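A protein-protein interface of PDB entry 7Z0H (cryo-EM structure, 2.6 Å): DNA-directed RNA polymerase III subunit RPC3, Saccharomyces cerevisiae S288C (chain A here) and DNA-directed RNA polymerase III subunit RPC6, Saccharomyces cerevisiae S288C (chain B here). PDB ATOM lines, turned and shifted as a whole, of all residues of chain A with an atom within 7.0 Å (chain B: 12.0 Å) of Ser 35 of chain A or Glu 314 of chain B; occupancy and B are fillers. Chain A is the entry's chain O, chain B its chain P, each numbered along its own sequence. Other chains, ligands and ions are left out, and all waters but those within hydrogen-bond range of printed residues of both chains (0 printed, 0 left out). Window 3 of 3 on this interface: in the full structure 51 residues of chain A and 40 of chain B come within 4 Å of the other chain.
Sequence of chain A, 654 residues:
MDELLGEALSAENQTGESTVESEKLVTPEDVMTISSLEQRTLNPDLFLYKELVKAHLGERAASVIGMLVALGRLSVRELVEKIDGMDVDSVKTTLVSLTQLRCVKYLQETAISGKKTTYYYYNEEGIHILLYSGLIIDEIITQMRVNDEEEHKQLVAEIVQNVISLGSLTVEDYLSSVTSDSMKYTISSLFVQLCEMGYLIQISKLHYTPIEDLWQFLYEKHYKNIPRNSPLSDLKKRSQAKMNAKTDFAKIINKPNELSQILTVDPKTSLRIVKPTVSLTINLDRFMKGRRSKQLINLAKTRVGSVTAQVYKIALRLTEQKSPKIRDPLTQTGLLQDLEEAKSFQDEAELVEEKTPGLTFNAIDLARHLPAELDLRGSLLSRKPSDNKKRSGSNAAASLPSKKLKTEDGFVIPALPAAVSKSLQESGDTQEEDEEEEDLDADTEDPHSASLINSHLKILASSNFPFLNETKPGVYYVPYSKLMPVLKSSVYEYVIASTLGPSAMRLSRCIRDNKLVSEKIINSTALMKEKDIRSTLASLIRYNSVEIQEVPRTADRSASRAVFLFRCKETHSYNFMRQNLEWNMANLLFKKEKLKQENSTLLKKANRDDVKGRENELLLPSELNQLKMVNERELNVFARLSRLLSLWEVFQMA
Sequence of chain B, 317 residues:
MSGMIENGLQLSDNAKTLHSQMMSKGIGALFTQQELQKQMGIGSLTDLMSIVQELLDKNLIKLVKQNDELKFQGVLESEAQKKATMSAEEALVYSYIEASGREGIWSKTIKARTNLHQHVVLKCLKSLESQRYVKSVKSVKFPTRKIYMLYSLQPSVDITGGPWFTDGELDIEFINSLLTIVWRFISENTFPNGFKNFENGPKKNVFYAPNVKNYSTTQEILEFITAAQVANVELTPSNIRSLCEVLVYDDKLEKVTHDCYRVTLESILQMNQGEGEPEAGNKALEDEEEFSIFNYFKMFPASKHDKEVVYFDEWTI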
ATOM      1  N   VAL A  26     -12.037  29.559  -6.974  1.00  0.00           N
ATOM      2  CA  VAL A  26     -11.366  29.950  -5.739  1.00  0.00           C
ATOM      3  C   VAL A  26      -9.863  29.742  -5.890  1.00  0.00           C
ATOM      4  O   VAL A  26      -9.407  28.698  -6.374  1.00  0.00           O
ATOM      5  CB  VAL A  26     -11.933  29.180  -4.532  1.00  0.00           C
ATOM      6  CG1 VAL A  26     -11.580  27.695  -4.584  1.00  0.00           C
ATOM      7  CG2 VAL A  26     -11.463  29.814  -3.232  1.00  0.00           C
ATOM      8  N   PRO A  28      -5.999  29.086  -4.861  1.00  0.00           N
ATOM      9  CA  PRO A  28      -5.298  28.334  -3.807  1.00  0.00           C
ATOM     10  C   PRO A  28      -4.761  29.226  -2.703  1.00  0.00           C
ATOM     11  O   PRO A  28      -4.720  28.803  -1.540  1.00  0.00           O
ATOM     12  CB  PRO A  28      -4.169  27.629  -4.572  1.00  0.00           C
ATOM     13  CG  PRO A  28      -4.687  27.507  -5.962  1.00  0.00           C
ATOM     14  CD  PRO A  28      -5.507  28.742  -6.207  1.00  0.00           C
ATOM     15  N   ASP A  30      -6.388  31.925  -1.858  1.00  0.00           N
ATOM     16  CA  ASP A  30      -7.608  32.314  -1.157  1.00  0.00           C
ATOM     17  C   ASP A  30      -8.016  31.256  -0.139  1.00  0.00           C
ATOM     18  O   ASP A  30      -8.303  31.573   1.021  1.00  0.00           O
ATOM     19  CB  ASP A  30      -8.733  32.564  -2.162  1.00  0.00           C
ATOM     20  CG  ASP A  30      -8.616  33.915  -2.842  1.00  0.00           C
ATOM     21  OD1 ASP A  30      -7.553  34.557  -2.707  1.00  0.00           O
ATOM     22  OD2 ASP A  30      -9.584  34.331  -3.513  1.00  0.00           O
ATOM     23  N   VAL A  31      -8.042  29.985  -0.553  1.00  0.00           N
ATOM     24  CA  VAL A  31      -8.281  28.918   0.411  1.00  0.00           C
ATOM     25  C   VAL A  31      -7.062  28.761   1.316  1.00  0.00           C
ATOM     26  O   VAL A  31      -5.989  29.327   1.071  1.00  0.00           O
ATOM     27  CB  VAL A  31      -8.633  27.591  -0.283  1.00  0.00           C
ATOM     28  CG1 VAL A  31     -10.063  27.616  -0.803  1.00  0.00           C
ATOM     29  CG2 VAL A  31      -7.660  27.294  -1.401  1.00  0.00           C
ATOM     30  N   MET A  32      -7.254  28.007   2.401  1.00  0.00           N
ATOM     31  CA  MET A  32      -6.243  27.740   3.425  1.00  0.00           C
ATOM     32  C   MET A  32      -5.922  28.996   4.230  1.00  0.00           C
ATOM     33  O   MET A  32      -5.146  28.951   5.190  1.00  0.00           O
ATOM     34  CB  MET A  32      -4.971  27.164   2.802  1.00  0.00           C
ATOM     35  CG  MET A  32      -4.012  26.515   3.786  1.00  0.00           C
ATOM     36  SD  MET A  32      -2.513  26.037   2.927  1.00  0.00           S
ATOM     37  CE  MET A  32      -3.198  25.744   1.304  1.00  0.00           C
ATOM     38  N   THR A  33      -6.518  30.118   3.850  1.00  0.00           N
ATOM     39  CA  THR A  33      -6.492  31.337   4.646  1.00  0.00           C
ATOM     40  C   THR A  33      -7.870  31.711   5.163  1.00  0.00           C
ATOM     41  O   THR A  33      -8.013  32.061   6.336  1.00  0.00           O
ATOM     42  CB  THR A  33      -5.920  32.499   3.825  1.00  0.00           C
ATOM     43  OG1 THR A  33      -4.606  32.157   3.366  1.00  0.00           O
ATOM     44  CG2 THR A  33      -5.837  33.758   4.672  1.00  0.00           C
ATOM     45  N   ILE A  34      -8.885  31.629   4.308  1.00  0.00           N
ATOM     46  CA  ILE A  34     -10.271  31.737   4.738  1.00  0.00           C
ATOM     47  C   ILE A  34     -10.967  30.378   4.768  1.00  0.00           C
ATOM     48  O   ILE A  34     -12.022  30.255   5.411  1.00  0.00           O
ATOM     49  CB  ILE A  34     -11.051  32.726   3.845  1.00  0.00           C
ATOM     50  CG1 ILE A  34     -12.389  33.114   4.482  1.00  0.00           C
ATOM     51  CG2 ILE A  34     -11.269  32.136   2.456  1.00  0.00           C
ATOM     52  CD1 ILE A  34     -13.005  34.364   3.896  1.00  0.00           C
ATOM     53  N   SER A  35     -10.404  29.352   4.124  1.00  0.00           N
ATOM     54  CA  SER A  35     -11.040  28.041   4.079  1.00  0.00           C
ATOM     55  C   SER A  35     -10.651  27.148   5.249  1.00  0.00           C
ATOM     56  O   SER A  35     -11.361  26.172   5.521  1.00  0.00           O
ATOM     57  CB  SER A  35     -10.688  27.329   2.773  1.00  0.00           C
ATOM     58  OG  SER A  35      -9.333  26.918   2.775  1.00  0.00           O
ATOM     59  N   SER A  36      -9.549  27.452   5.935  1.00  0.00           N
ATOM     60  CA  SER A  36      -9.072  26.656   7.068  1.00  0.00           C
ATOM     61  C   SER A  36      -8.813  25.205   6.665  1.00  0.00           C
ATOM     62  O   SER A  36      -9.259  24.263   7.322  1.00  0.00           O
ATOM     63  CB  SER A  36     -10.051  26.729   8.243  1.00  0.00           C
ATOM     64  OG  SER A  36      -9.466  26.215   9.425  1.00  0.00           O
ATOM     65  N   LEU A  37      -8.085  25.024   5.562  1.00  0.00           N
ATOM     66  CA  LEU A  37      -7.776  23.674   5.107  1.00  0.00           C
ATOM     67  C   LEU A  37      -6.596  23.084   5.871  1.00  0.00           C
ATOM     68  O   LEU A  37      -6.548  21.869   6.089  1.00  0.00           O
ATOM     69  CB  LEU A  37      -7.526  23.695   3.594  1.00  0.00           C
ATOM     70  CG  LEU A  37      -7.606  22.494   2.641  1.00  0.00           C
ATOM     71  CD1 LEU A  37      -7.139  22.959   1.274  1.00  0.00           C
ATOM     72  CD2 LEU A  37      -6.801  21.272   3.078  1.00  0.00           C
ATOM     73  N   GLU A  38      -5.658  23.924   6.318  1.00  0.00           N
ATOM     74  CA  GLU A  38      -4.525  23.412   7.083  1.00  0.00           C
ATOM     75  C   GLU A  38      -4.940  22.965   8.479  1.00  0.00           C
ATOM     76  O   GLU A  38      -4.262  22.125   9.084  1.00  0.00           O
ATOM     77  CB  GLU A  38      -3.418  24.468   7.162  1.00  0.00           C
ATOM     78  CG  GLU A  38      -3.670  25.599   8.153  1.00  0.00           C
ATOM     79  CD  GLU A  38      -4.594  26.673   7.607  1.00  0.00           C
ATOM     80  OE1 GLU A  38      -5.485  26.350   6.794  1.00  0.00           O
ATOM     81  OE2 GLU A  38      -4.429  27.847   7.999  1.00  0.00           O
ATOM     82  N   GLN A  39      -6.043  23.502   9.006  1.00  0.00           N
ATOM     83  CA  GLN A  39      -6.545  23.043  10.296  1.00  0.00           C
ATOM     84  C   GLN A  39      -7.280  21.713  10.192  1.00  0.00           C
ATOM     85  O   GLN A  39      -7.463  21.039  11.211  1.00  0.00           O
ATOM     86  CB  GLN A  39      -7.475  24.089  10.913  1.00  0.00           C
ATOM     87  CG  GLN A  39      -6.766  25.254  11.586  1.00  0.00           C
ATOM     88  CD  GLN A  39      -6.587  26.439  10.661  1.00  0.00           C
ATOM     89  OE1 GLN A  39      -6.988  26.397   9.499  1.00  0.00           O
ATOM     90  NE2 GLN A  39      -5.991  27.507  11.175  1.00  0.00           N
ATOM     91  N   ARG A  40      -7.698  21.317   8.987  1.00  0.00           N
ATOM     92  CA  ARG A  40      -8.471  20.092   8.828  1.00  0.00           C
ATOM     93  C   ARG A  40      -7.615  18.841   8.972  1.00  0.00           C
ATOM     94  O   ARG A  40      -8.163  17.744   9.125  1.00  0.00           O
ATOM     95  CB  ARG A  40      -9.174  20.093   7.470  1.00  0.00           C
ATOM     96  CG  ARG A  40     -10.291  21.121   7.354  1.00  0.00           C
ATOM     97  CD  ARG A  40     -10.799  21.225   5.926  1.00  0.00           C
ATOM     98  NE  ARG A  40     -11.329  22.551   5.631  1.00  0.00           N
ATOM     99  CZ  ARG A  40     -11.407  23.071   4.414  1.00  0.00           C
ATOM    100  NH1 ARG A  40     -11.003  22.400   3.348  1.00  0.00           N
ATOM    101  NH2 ARG A  40     -11.901  24.297   4.262  1.00  0.00           N
ATOM    102  N   TYR A 543     -19.192   9.815   6.537  1.00  0.00           N
ATOM    103  CA  TYR A 543     -18.860   9.664   7.944  1.00  0.00           C
ATOM    104  C   TYR A 543     -18.675   8.184   8.278  1.00  0.00           C
ATOM    105  O   TYR A 543     -18.701   7.312   7.405  1.00  0.00           O
ATOM    106  CB  TYR A 543     -19.944  10.296   8.815  1.00  0.00           C
ATOM    107  CG  TYR A 543     -20.193  11.766   8.542  1.00  0.00           C
ATOM    108  CD1 TYR A 543     -19.219  12.561   7.952  1.00  0.00           C
ATOM    109  CD2 TYR A 543     -21.404  12.357   8.878  1.00  0.00           C
ATOM    110  CE1 TYR A 543     -19.444  13.903   7.703  1.00  0.00           C
ATOM    111  CE2 TYR A 543     -21.637  13.698   8.634  1.00  0.00           C
ATOM    112  CZ  TYR A 543     -20.654  14.465   8.046  1.00  0.00           C
ATOM    113  OH  TYR A 543     -20.881  15.799   7.799  1.00  0.00           O
ATOM    114  N   ASN A 580     -14.976  14.718  15.161  1.00  0.00           N
ATOM    115  CA  ASN A 580     -15.611  15.882  14.543  1.00  0.00           C
ATOM    116  C   ASN A 580     -15.948  16.946  15.583  1.00  0.00           C
ATOM    117  O   ASN A 580     -15.657  18.132  15.392  1.00  0.00           O
ATOM    118  CB  ASN A 580     -16.867  15.458  13.779  1.00  0.00           C
ATOM    119  CG  ASN A 580     -17.444  16.580  12.925  1.00  0.00           C
ATOM    120  OD1 ASN A 580     -16.896  17.681  12.865  1.00  0.00           O
ATOM    121  ND2 ASN A 580     -18.557  16.299  12.258  1.00  0.00           N
ATOM    122  N   TRP A 583     -12.754  18.487  17.120  1.00  0.00           N
ATOM    123  CA  TRP A 583     -12.167  19.381  16.130  1.00  0.00           C
ATOM    124  C   TRP A 583     -12.955  20.676  16.018  1.00  0.00           C
ATOM    125  O   TRP A 583     -12.368  21.752  15.870  1.00  0.00           O
ATOM    126  CB  TRP A 583     -12.100  18.676  14.777  1.00  0.00           C
ATOM    127  CG  TRP A 583     -11.378  19.453  13.729  1.00  0.00           C
ATOM    128  CD1 TRP A 583     -10.028  19.566  13.575  1.00  0.00           C
ATOM    129  CD2 TRP A 583     -11.969  20.236  12.689  1.00  0.00           C
ATOM    130  NE1 TRP A 583      -9.742  20.368  12.496  1.00  0.00           N
ATOM    131  CE2 TRP A 583     -10.918  20.793  11.937  1.00  0.00           C
ATOM    132  CE3 TRP A 583     -13.287  20.518  12.319  1.00  0.00           C
ATOM    133  CZ2 TRP A 583     -11.143  21.616  10.837  1.00  0.00           C
ATOM    134  CZ3 TRP A 583     -13.508  21.336  11.228  1.00  0.00           C
ATOM    135  CH2 TRP A 583     -12.441  21.871  10.496  1.00  0.00           C
ATOM    136  N   ASN A 584     -14.286  20.595  16.067  1.00  0.00           N
ATOM    137  CA  ASN A 584     -15.098  21.806  16.005  1.00  0.00           C
ATOM    138  C   ASN A 584     -14.852  22.697  17.217  1.00  0.00           C
ATOM    139  O   ASN A 584     -14.718  23.919  17.079  1.00  0.00           O
ATOM    140  CB  ASN A 584     -16.576  21.435  15.894  1.00  0.00           C
ATOM    141  CG  ASN A 584     -16.930  20.858  14.537  1.00  0.00           C
ATOM    142  OD1 ASN A 584     -16.798  21.525  13.511  1.00  0.00           O
ATOM    143  ND2 ASN A 584     -17.377  19.608  14.526  1.00  0.00           N
ATOM    144  N   ASN A 587     -11.709  24.390  16.728  1.00  0.00           N
ATOM    145  CA  ASN A 587     -11.881  25.485  15.777  1.00  0.00           C
ATOM    146  C   ASN A 587     -12.452  26.725  16.452  1.00  0.00           C
ATOM    147  O   ASN A 587     -12.041  27.847  16.143  1.00  0.00           O
ATOM    148  CB  ASN A 587     -12.784  25.062  14.619  1.00  0.00           C
ATOM    149  CG  ASN A 587     -12.094  24.136  13.641  1.00  0.00           C
ATOM    150  OD1 ASN A 587     -12.470  24.074  12.474  1.00  0.00           O
ATOM    151  ND2 ASN A 587     -11.088  23.408  14.108  1.00  0.00           N
ATOM    152  N   ASP B 306     -21.715  36.377   8.821  1.00  0.00           N
ATOM    153  CA  ASP B 306     -20.775  36.452   9.927  1.00  0.00           C
ATOM    154  C   ASP B 306     -19.869  35.221   9.954  1.00  0.00           C
ATOM    155  O   ASP B 306     -19.936  34.340   9.092  1.00  0.00           O
ATOM    156  CB  ASP B 306     -21.530  36.605  11.245  1.00  0.00           C
ATOM    157  CG  ASP B 306     -22.636  35.579  11.406  1.00  0.00           C
ATOM    158  OD1 ASP B 306     -22.860  34.792  10.464  1.00  0.00           O
ATOM    159  OD2 ASP B 306     -23.285  35.566  12.472  1.00  0.00           O
ATOM    160  N   LYS B 307     -19.011  35.162  10.967  1.00  0.00           N
ATOM    161  CA  LYS B 307     -18.009  34.122  11.114  1.00  0.00           C
ATOM    162  C   LYS B 307     -18.340  33.241  12.316  1.00  0.00           C
ATOM    163  O   LYS B 307     -19.410  33.359  12.927  1.00  0.00           O
ATOM    164  CB  LYS B 307     -16.619  34.748  11.236  1.00  0.00           C
ATOM    165  CG  LYS B 307     -15.987  35.124   9.907  1.00  0.00           C
ATOM    166  CD  LYS B 307     -16.360  36.543   9.513  1.00  0.00           C
ATOM    167  CE  LYS B 307     -15.717  37.556  10.443  1.00  0.00           C
ATOM    168  NZ  LYS B 307     -16.056  38.954  10.066  1.00  0.00           N
ATOM    169  N   GLU B 308     -17.413  32.339  12.643  1.00  0.00           N
ATOM    170  CA  GLU B 308     -17.511  31.374  13.736  1.00  0.00           C
ATOM    171  C   GLU B 308     -18.611  30.347  13.508  1.00  0.00           C
ATOM    172  O   GLU B 308     -18.911  29.559  14.416  1.00  0.00           O
ATOM    173  CB  GLU B 308     -17.728  32.057  15.093  1.00  0.00           C
ATOM    174  CG  GLU B 308     -16.530  32.838  15.607  1.00  0.00           C
ATOM    175  CD  GLU B 308     -16.297  34.127  14.847  1.00  0.00           C
ATOM    176  OE1 GLU B 308     -17.177  35.012  14.897  1.00  0.00           O
ATOM    177  OE2 GLU B 308     -15.236  34.256  14.200  1.00  0.00           O
ATOM    178  N   VAL B 309     -19.216  30.326  12.321  1.00  0.00           N
ATOM    179  CA  VAL B 309     -20.293  29.388  12.037  1.00  0.00           C
ATOM    180  C   VAL B 309     -19.718  27.984  11.929  1.00  0.00           C
ATOM    181  O   VAL B 309     -18.707  27.758  11.251  1.00  0.00           O
ATOM    182  CB  VAL B 309     -21.034  29.794  10.754  1.00  0.00           C
ATOM    183  CG1 VAL B 309     -22.272  28.933  10.559  1.00  0.00           C
ATOM    184  CG2 VAL B 309     -21.401  31.270  10.800  1.00  0.00           C
ATOM    185  N   VAL B 310     -20.360  27.033  12.597  1.00  0.00           N
ATOM    186  CA  VAL B 310     -19.870  25.664  12.677  1.00  0.00           C
ATOM    187  C   VAL B 310     -20.593  24.819  11.640  1.00  0.00           C
ATOM    188  O   VAL B 310     -21.757  25.069  11.302  1.00  0.00           O
ATOM    189  CB  VAL B 310     -20.059  25.092  14.098  1.00  0.00           C
ATOM    190  CG1 VAL B 310     -19.259  23.807  14.276  1.00  0.00           C
ATOM    191  CG2 VAL B 310     -19.676  26.127  15.141  1.00  0.00           C
ATOM    192  N   TYR B 311     -19.893  23.816  11.117  1.00  0.00           N
ATOM    193  CA  TYR B 311     -20.449  22.910  10.122  1.00  0.00           C
ATOM    194  C   TYR B 311     -19.991  21.494  10.435  1.00  0.00           C
ATOM    195  O   TYR B 311     -18.812  21.271  10.719  1.00  0.00           O
ATOM    196  CB  TYR B 311     -20.016  23.315   8.709  1.00  0.00           C
ATOM    197  CG  TYR B 311     -20.345  24.749   8.355  1.00  0.00           C
ATOM    198  CD1 TYR B 311     -19.449  25.776   8.623  1.00  0.00           C
ATOM    199  CD2 TYR B 311     -21.554  25.077   7.756  1.00  0.00           C
ATOM    200  CE1 TYR B 311     -19.749  27.089   8.305  1.00  0.00           C
ATOM    201  CE2 TYR B 311     -21.862  26.383   7.433  1.00  0.00           C
ATOM    202  CZ  TYR B 311     -20.957  27.384   7.708  1.00  0.00           C
ATOM    203  OH  TYR B 311     -21.263  28.687   7.386  1.00  0.00           O
ATOM    204  N   PHE B 312     -20.925  20.539  10.385  1.00  0.00           N
ATOM    205  CA  PHE B 312     -20.584  19.153  10.685  1.00  0.00           C
ATOM    206  C   PHE B 312     -19.805  18.487   9.560  1.00  0.00           C
ATOM    207  O   PHE B 312     -19.213  17.425   9.779  1.00  0.00           O
ATOM    208  CB  PHE B 312     -21.848  18.348  10.990  1.00  0.00           C
ATOM    209  CG  PHE B 312     -22.299  18.448  12.420  1.00  0.00           C
ATOM    210  CD1 PHE B 312     -21.472  18.999  13.386  1.00  0.00           C
ATOM    211  CD2 PHE B 312     -23.545  17.981  12.800  1.00  0.00           C
ATOM    212  CE1 PHE B 312     -21.886  19.089  14.703  1.00  0.00           C
ATOM    213  CE2 PHE B 312     -23.965  18.069  14.116  1.00  0.00           C
ATOM    214  CZ  PHE B 312     -23.133  18.624  15.068  1.00  0.00           C
ATOM    215  N   ASP B 313     -19.797  19.076   8.367  1.00  0.00           N
ATOM    216  CA  ASP B 313     -19.012  18.570   7.250  1.00  0.00           C
ATOM    217  C   ASP B 313     -17.670  19.275   7.110  1.00  0.00           C
ATOM    218  O   ASP B 313     -16.931  18.991   6.162  1.00  0.00           O
ATOM    219  CB  ASP B 313     -19.810  18.699   5.948  1.00  0.00           C
ATOM    220  CG  ASP B 313     -20.394  20.085   5.756  1.00  0.00           C
ATOM    221  OD1 ASP B 313     -20.211  20.937   6.648  1.00  0.00           O
ATOM    222  OD2 ASP B 313     -21.039  20.322   4.714  1.00  0.00           O
ATOM    223  N   GLU B 314     -17.340  20.183   8.031  1.00  0.00           N
ATOM    224  CA  GLU B 314     -16.082  20.916   7.940  1.00  0.00           C
ATOM    225  C   GLU B 314     -14.885  19.994   8.136  1.00  0.00           C
ATOM    226  O   GLU B 314     -13.836  20.185   7.508  1.00  0.00           O
ATOM    227  CB  GLU B 314     -16.063  22.045   8.971  1.00  0.00           C
ATOM    228  CG  GLU B 314     -15.133  23.193   8.625  1.00  0.00           C
ATOM    229  CD  GLU B 314     -15.529  23.894   7.341  1.00  0.00           C
ATOM    230  OE1 GLU B 314     -16.739  23.931   7.032  1.00  0.00           O
ATOM    231  OE2 GLU B 314     -14.630  24.404   6.641  1.00  0.00           O
ATOM    232  N   TRP B 315     -15.021  18.991   9.005  1.00  0.00           N
ATOM    233  CA  TRP B 315     -13.937  18.053   9.266  1.00  0.00           C
ATOM    234  C   TRP B 315     -13.721  17.067   8.125  1.00  0.00           C
ATOM    235  O   TRP B 315     -12.702  16.369   8.116  1.00  0.00           O
ATOM    236  CB  TRP B 315     -14.216  17.298  10.567  1.00  0.00           C
ATOM    237  CG  TRP B 315     -13.055  16.515  11.086  1.00  0.00           C
ATOM    238  CD1 TRP B 315     -11.866  17.009  11.533  1.00  0.00           C
ATOM    239  CD2 TRP B 315     -12.975  15.092  11.221  1.00  0.00           C
ATOM    240  NE1 TRP B 315     -11.047  15.982  11.934  1.00  0.00           N
ATOM    241  CE2 TRP B 315     -11.706  14.794  11.753  1.00  0.00           C
ATOM    242  CE3 TRP B 315     -13.853  14.042  10.941  1.00  0.00           C
ATOM    243  CZ2 TRP B 315     -11.294  13.491  12.012  1.00  0.00           C
ATOM    244  CZ3 TRP B 315     -13.443  12.749  11.197  1.00  0.00           C
ATOM    245  CH2 TRP B 315     -12.175  12.484  11.726  1.00  0.00           C
ATOM    246  N   THR B 316     -14.643  16.996   7.169  1.00  0.00           N
ATOM    247  CA  THR B 316     -14.501  16.097   6.029  1.00  0.00           C
ATOM    248  C   THR B 316     -15.318  16.588   4.838  1.00  0.00           C
ATOM    249  O   THR B 316     -14.884  17.467   4.093  1.00  0.00           O
ATOM    250  CB  THR B 316     -14.937  14.664   6.381  1.00  0.00           C
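NH2 of Arg 40 of chain A lies within salt-bridge range of OE2 of Glu 314 of chain B (3.6 Å).
The backbone carbonyl oxygen (O) of Phe 312 of chain B is in hydrogen-bond range of the side-chain hydroxyl (OH) of Tyr 543 of chain A (3.1 Å).
The backbone NH (N) of Asp 313 of chain B lies close to the side-chain hydroxyl (OH) of Tyr 543 of chain A, at 3.5 Å.
The backbone carbonyl oxygen (O) of Phe 312 of chain B is in hydrogen-bond range of the side-chain amide nitrogen (ND2) of Asn 580 of chain A (2.8 Å).
The side-chain amide oxygen (OD1) of Asn 584 of chain A lies close to the backbone carbonyl oxygen (O) of Tyr 311 of chain B, at 3.5 Å.
The backbone carbonyl oxygen (O) of Ser 36 of chain A lies within hydrogen-bond range of the guanidinium group (NE) of Arg 40 of chain A (3.2 Å).
The backbone carbonyl oxygen (O) of Gln 39 of chain A is in hydrogen-bond range of the indole nitrogen (NE1) of Trp 583 of chain A, 2.7 Å away.
The backbone carbonyl oxygen (O) of Asn 580 of chain A lies within hydrogen-bond range of the side-chain amide nitrogen (ND2) of Asn 584 of chain A (2.4 Å).
ND2 of Asn 587 of chain A is in hydrogen-bond range of O of Trp 583 of chain A (2.7 Å).
Among the printed residues, pairs that only touch across the chains: Trp 583 of chain A with Trp 315 of chain B (3.3 Å), Asn 584 of chain A with Val 310 of chain B (3.4 Å), Trp 583 of chain A with Glu 314 of chain B (3.5 Å), Asn 580 of chain A with Trp 315 of chain B (3.6 Å) and Ser 35 of chain A with Glu 314 of chain B (3.9 Å).
Of chain B, only Glu 314 comes within 4 Å of Ser 35 of chain A.
Of chain A, only Ser 35, Arg 40 and Trp 583 come within 4 Å of Glu 314 of chain B.
No residue of chain B comes within 4 Å of Met 32 of chain A.
No residue of chain B comes within 4 Å of Thr 33 of chain A.
No residue of chain B comes within 4 Å of Ile 34 of chain A.
No residue of chain B comes within 4 Å of Ser 36 of chain A.
No residue of chain B comes within 4 Å of Leu 37 of chain A.
Gln 39 of chain A touches none of the printed residues of chain B.
Printed residues of chain B within 4 Å of Arg 40 of chain A: Glu 314 (3.6 Å).
Of the printed residues of chain B, Tyr 543 of chain A touches Phe 312 (3.1 Å) and Asp 313 (3.4 Å).
Of the printed residues of chain B, Asn 580 of chain A touches Phe 312 (2.8 Å) and Trp 315 (3.6 Å).
Printed residues of chain A within 4 Å of Asp 313 of chain B: Tyr 543.
Asp 30 of chain A touches none of the printed residues of chain B.
The nearest residue of chain B that does not touch Ser 35 of chain A is Tyr 311 of chain B (8.7 Å).
Hydrophobic or aromatic side chains of chain B within 4 Å of the printed part of chain A: Val 310 and Trp 315.
Along chain B the printed residues that touch a printed residue of chain A span positions 310 to 315.
Along chain A the printed residues that touch a printed residue of chain B span positions 35 to 584.
Among the printed residues, Asp or Glu carboxylates within 4 Å of a Lys or Arg side-chain nitrogen of the other chain: Arg 40 of chain A with Glu 314 of chain B (3.6 Å).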
